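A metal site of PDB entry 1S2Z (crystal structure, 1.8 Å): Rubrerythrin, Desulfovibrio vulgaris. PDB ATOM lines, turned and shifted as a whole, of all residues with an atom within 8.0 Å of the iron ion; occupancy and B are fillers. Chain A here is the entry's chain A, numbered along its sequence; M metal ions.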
ATOM      1  N   ARG A 157      -6.829   4.388   3.615  1.00  0.00           N
ATOM      2  CA  ARG A 157      -7.093   5.364   4.672  1.00  0.00           C
ATOM      3  C   ARG A 157      -6.658   6.759   4.282  1.00  0.00           C
ATOM      4  O   ARG A 157      -5.593   6.954   3.710  1.00  0.00           O
ATOM      5  CB  ARG A 157      -6.382   4.959   5.970  1.00  0.00           C
ATOM      6  CG  ARG A 157      -6.789   5.823   7.170  1.00  0.00           C
ATOM      7  CD  ARG A 157      -5.949   5.533   8.407  1.00  0.00           C
ATOM      8  NE  ARG A 157      -4.577   6.022   8.276  1.00  0.00           N
ATOM      9  CZ  ARG A 157      -3.977   6.834   9.143  1.00  0.00           C
ATOM     10  NH1 ARG A 157      -4.614   7.260  10.217  1.00  0.00           N
ATOM     11  NH2 ARG A 157      -2.724   7.222   8.920  1.00  0.00           N
ATOM     12  N   CYS A 158      -7.514   7.743   4.580  1.00  0.00           N
ATOM     13  CA  CYS A 158      -7.188   9.132   4.300  1.00  0.00           C
ATOM     14  C   CYS A 158      -6.297   9.596   5.458  1.00  0.00           C
ATOM     15  O   CYS A 158      -6.719   9.574   6.608  1.00  0.00           O
ATOM     16  CB  CYS A 158      -8.456   9.985   4.264  1.00  0.00           C
ATOM     17  SG  CYS A 158      -8.132  11.756   4.136  1.00  0.00           S
ATOM     18  N   ARG A 159      -5.068  10.018   5.155  1.00  0.00           N
ATOM     19  CA  ARG A 159      -4.168  10.472   6.219  1.00  0.00           C
ATOM     20  C   ARG A 159      -4.623  11.776   6.858  1.00  0.00           C
ATOM     21  O   ARG A 159      -4.305  12.059   8.015  1.00  0.00           O
ATOM     22  CB  ARG A 159      -2.739  10.635   5.661  1.00  0.00           C
ATOM     23  CG  ARG A 159      -2.034   9.323   5.366  1.00  0.00           C
ATOM     24  CD  ARG A 159      -0.604   9.564   4.876  1.00  0.00           C
ATOM     25  NE  ARG A 159       0.234  10.198   5.895  1.00  0.00           N
ATOM     26  CZ  ARG A 159       0.672   9.602   6.993  1.00  0.00           C
ATOM     27  NH1 ARG A 159       0.352   8.332   7.253  1.00  0.00           N
ATOM     28  NH2 ARG A 159       1.416  10.272   7.857  1.00  0.00           N
ATOM     29  N   ASN A 160      -5.401  12.571   6.119  1.00  0.00           N
ATOM     30  CA  ASN A 160      -5.874  13.849   6.624  1.00  0.00           C
ATOM     31  C   ASN A 160      -6.972  13.734   7.703  1.00  0.00           C
ATOM     32  O   ASN A 160      -6.921  14.464   8.701  1.00  0.00           O
ATOM     33  CB  ASN A 160      -6.390  14.705   5.467  1.00  0.00           C
ATOM     34  CG  ASN A 160      -6.750  16.117   5.890  1.00  0.00           C
ATOM     35  OD1 ASN A 160      -7.918  16.523   5.847  1.00  0.00           O
ATOM     36  ND2 ASN A 160      -5.742  16.879   6.301  1.00  0.00           N
ATOM     37  N   CYS A 161      -7.926  12.834   7.516  1.00  0.00           N
ATOM     38  CA  CYS A 161      -9.029  12.699   8.469  1.00  0.00           C
ATOM     39  C   CYS A 161      -9.323  11.298   8.987  1.00  0.00           C
ATOM     40  O   CYS A 161     -10.160  11.135   9.889  1.00  0.00           O
ATOM     41  CB  CYS A 161     -10.314  13.260   7.845  1.00  0.00           C
ATOM     42  SG  CYS A 161     -11.084  12.149   6.623  1.00  0.00           S
ATOM     43  N   GLY A 162      -8.671  10.282   8.427  1.00  0.00           N
ATOM     44  CA  GLY A 162      -8.900   8.930   8.906  1.00  0.00           C
ATOM     45  C   GLY A 162     -10.009   8.153   8.216  1.00  0.00           C
ATOM     46  O   GLY A 162     -10.292   7.024   8.595  1.00  0.00           O
ATOM     47  N   TYR A 163     -10.653   8.763   7.222  1.00  0.00           N
ATOM     48  CA  TYR A 163     -11.721   8.057   6.508  1.00  0.00           C
ATOM     49  C   TYR A 163     -11.151   6.788   5.886  1.00  0.00           C
ATOM     50  O   TYR A 163     -10.024   6.784   5.397  1.00  0.00           O
ATOM     51  CB  TYR A 163     -12.312   8.935   5.404  1.00  0.00           C
ATOM     52  CG  TYR A 163     -13.373   8.231   4.590  1.00  0.00           C
ATOM     53  CD1 TYR A 163     -14.631   7.957   5.123  1.00  0.00           C
ATOM     54  CD2 TYR A 163     -13.095   7.782   3.297  1.00  0.00           C
ATOM     55  CE1 TYR A 163     -15.597   7.267   4.391  1.00  0.00           C
ATOM     56  CE2 TYR A 163     -14.054   7.094   2.552  1.00  0.00           C
ATOM     57  CZ  TYR A 163     -15.301   6.843   3.111  1.00  0.00           C
ATOM     58  OH  TYR A 163     -16.246   6.160   2.375  1.00  0.00           O
ATOM     59  N   VAL A 164     -11.931   5.709   5.905  1.00  0.00           N
ATOM     60  CA  VAL A 164     -11.506   4.449   5.322  1.00  0.00           C
ATOM     61  C   VAL A 164     -12.380   4.142   4.109  1.00  0.00           C
ATOM     62  O   VAL A 164     -13.609   4.129   4.198  1.00  0.00           O
ATOM     63  CB  VAL A 164     -11.630   3.293   6.332  1.00  0.00           C
ATOM     64  CG1 VAL A 164     -11.299   1.958   5.658  1.00  0.00           C
ATOM     65  CG2 VAL A 164     -10.691   3.522   7.511  1.00  0.00           C
ATOM     66  N   LEU A 173     -11.587  12.126  -4.358  1.00  0.00           N
ATOM     67  CA  LEU A 173     -11.809  13.051  -3.255  1.00  0.00           C
ATOM     68  C   LEU A 173     -12.273  12.274  -2.028  1.00  0.00           C
ATOM     69  O   LEU A 173     -13.090  11.354  -2.156  1.00  0.00           O
ATOM     70  CB  LEU A 173     -12.874  14.091  -3.616  1.00  0.00           C
ATOM     71  CG  LEU A 173     -12.501  15.153  -4.648  1.00  0.00           C
ATOM     72  CD1 LEU A 173     -13.711  16.057  -4.896  1.00  0.00           C
ATOM     73  CD2 LEU A 173     -11.324  15.961  -4.135  1.00  0.00           C
ATOM     74  N   CYS A 174     -11.763  12.643  -0.863  1.00  0.00           N
ATOM     75  CA  CYS A 174     -12.185  11.974   0.361  1.00  0.00           C
ATOM     76  C   CYS A 174     -13.614  12.445   0.643  1.00  0.00           C
ATOM     77  O   CYS A 174     -13.877  13.641   0.715  1.00  0.00           O
ATOM     78  CB  CYS A 174     -11.283  12.368   1.537  1.00  0.00           C
ATOM     79  SG  CYS A 174     -11.821  11.646   3.112  1.00  0.00           S
ATOM     80  N   PRO A 175     -14.554  11.509   0.802  1.00  0.00           N
ATOM     81  CA  PRO A 175     -15.931  11.933   1.064  1.00  0.00           C
ATOM     82  C   PRO A 175     -16.146  12.601   2.437  1.00  0.00           C
ATOM     83  O   PRO A 175     -17.152  13.280   2.646  1.00  0.00           O
ATOM     84  CB  PRO A 175     -16.734  10.640   0.904  1.00  0.00           C
ATOM     85  CG  PRO A 175     -15.766   9.598   1.352  1.00  0.00           C
ATOM     86  CD  PRO A 175     -14.465  10.036   0.713  1.00  0.00           C
ATOM     87  N   ALA A 176     -15.202  12.405   3.341  1.00  0.00           N
ATOM     88  CA  ALA A 176     -15.312  12.977   4.682  1.00  0.00           C
ATOM     89  C   ALA A 176     -14.692  14.378   4.804  1.00  0.00           C
ATOM     90  O   ALA A 176     -15.319  15.289   5.345  1.00  0.00           O
ATOM     91  CB  ALA A 176     -14.680  12.036   5.709  1.00  0.00           C
ATOM     92  N   CYS A 177     -13.461  14.552   4.314  1.00  0.00           N
ATOM     93  CA  CYS A 177     -12.799  15.850   4.434  1.00  0.00           C
ATOM     94  C   CYS A 177     -12.602  16.605   3.123  1.00  0.00           C
ATOM     95  O   CYS A 177     -12.061  17.708   3.113  1.00  0.00           O
ATOM     96  CB  CYS A 177     -11.446  15.689   5.128  1.00  0.00           C
ATOM     97  SG  CYS A 177     -10.184  14.894   4.120  1.00  0.00           S
ATOM     98  N   ALA A 178     -13.040  16.009   2.018  1.00  0.00           N
ATOM     99  CA  ALA A 178     -12.938  16.618   0.694  1.00  0.00           C
ATOM    100  C   ALA A 178     -11.522  16.838   0.169  1.00  0.00           C
ATOM    101  O   ALA A 178     -11.340  17.532  -0.838  1.00  0.00           O
ATOM    102  CB  ALA A 178     -13.710  17.947   0.676  1.00  0.00           C
ATOM    103  N   HIS A 179     -10.526  16.289   0.848  1.00  0.00           N
ATOM    104  CA  HIS A 179      -9.154  16.443   0.371  1.00  0.00           C
ATOM    105  C   HIS A 179      -8.912  15.463  -0.778  1.00  0.00           C
ATOM    106  O   HIS A 179      -9.592  14.447  -0.882  1.00  0.00           O
ATOM    107  CB  HIS A 179      -8.159  16.220   1.513  1.00  0.00           C
ATOM    108  CG  HIS A 179      -8.027  17.396   2.426  1.00  0.00           C
ATOM    109  ND1 HIS A 179      -9.110  17.990   3.039  1.00  0.00           N
ATOM    110  CD2 HIS A 179      -6.937  18.116   2.809  1.00  0.00           C
ATOM    111  CE1 HIS A 179      -8.699  19.022   3.761  1.00  0.00           C
ATOM    112  NE2 HIS A 179      -7.386  19.109   3.645  1.00  0.00           N
ATOM    113  N   PRO A 180      -7.949  15.766  -1.666  1.00  0.00           N
ATOM    114  CA  PRO A 180      -7.651  14.899  -2.810  1.00  0.00           C
ATOM    115  C   PRO A 180      -7.052  13.527  -2.519  1.00  0.00           C
ATOM    116  O   PRO A 180      -6.572  13.248  -1.425  1.00  0.00           O
ATOM    117  CB  PRO A 180      -6.737  15.762  -3.674  1.00  0.00           C
ATOM    118  CG  PRO A 180      -5.999  16.563  -2.658  1.00  0.00           C
ATOM    119  CD  PRO A 180      -7.088  16.963  -1.675  1.00  0.00           C
ATOM    120  N   HIS A 183      -3.906  12.188  -0.374  1.00  0.00           N
ATOM    121  CA  HIS A 183      -3.818  11.904   1.056  1.00  0.00           C
ATOM    122  C   HIS A 183      -4.042  10.454   1.458  1.00  0.00           C
ATOM    123  O   HIS A 183      -3.834  10.097   2.618  1.00  0.00           O
ATOM    124  CB  HIS A 183      -4.822  12.796   1.801  1.00  0.00           C
ATOM    125  CG  HIS A 183      -4.487  14.256   1.737  1.00  0.00           C
ATOM    126  ND1 HIS A 183      -3.748  14.898   2.715  1.00  0.00           N
ATOM    127  CD2 HIS A 183      -4.719  15.185   0.785  1.00  0.00           C
ATOM    128  CE1 HIS A 183      -3.537  16.149   2.364  1.00  0.00           C
ATOM    129  NE2 HIS A 183      -4.118  16.351   1.191  1.00  0.00           N
ATOM    130  N   PHE A 184      -4.431   9.612   0.503  1.00  0.00           N
ATOM    131  CA  PHE A 184      -4.693   8.214   0.814  1.00  0.00           C
ATOM    132  C   PHE A 184      -3.502   7.269   0.813  1.00  0.00           C
ATOM    133  O   PHE A 184      -2.531   7.452   0.071  1.00  0.00           O
ATOM    134  CB  PHE A 184      -5.772   7.659  -0.125  1.00  0.00           C
ATOM    135  CG  PHE A 184      -7.156   8.156   0.184  1.00  0.00           C
ATOM    136  CD1 PHE A 184      -7.610   9.373  -0.311  1.00  0.00           C
ATOM    137  CD2 PHE A 184      -8.008   7.407   1.008  1.00  0.00           C
ATOM    138  CE1 PHE A 184      -8.891   9.839  -0.002  1.00  0.00           C
ATOM    139  CE2 PHE A 184      -9.286   7.871   1.327  1.00  0.00           C
ATOM    140  CZ  PHE A 184      -9.724   9.088   0.816  1.00  0.00           C
HETATM  141 FE    FE M   1     -10.290  12.590   4.538  1.00  0.00          FE
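The nearest printed residue that does not touch the iron ion is Tyr 163 (4.3 Å).
The backbone NH of Cys 174 is in hydrogen-bond range of the backbone carbonyl oxygen of His 179 (2.8 Å). SG of Cys 174 lies close to N of Ala 176, at 3.5 Å. A ring nitrogen (ND1) of His 179 sits at hydrogen-bond distance from the backbone carbonyl oxygen of Cys 177 (3.0 Å). The backbone NH (N) of Tyr 163 sits close to the side-chain sulfur (SG) of Cys 161, at 3.5 Å. The backbone carbonyl oxygen of Tyr 163 lies within hydrogen-bond range of the backbone NH of Cys 158 (2.8 Å). The backbone NH (N) of Asn 160 lies close to the side-chain sulfur (SG) of Cys 158 (3.5 Å). The side-chain amide oxygen of Asn 160 sits close to the side-chain sulfur of Cys 177 (3.3 Å).
The iron ion is bound by the side-chain sulfur (SG) of Cys 161 (2.3 Å), the side-chain sulfur (SG) of Cys 174 (2.3 Å), the side-chain sulfur (SG) of Cys 177 (2.3 Å) and the side-chain sulfur (SG) of Cys 158 (2.3 Å).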
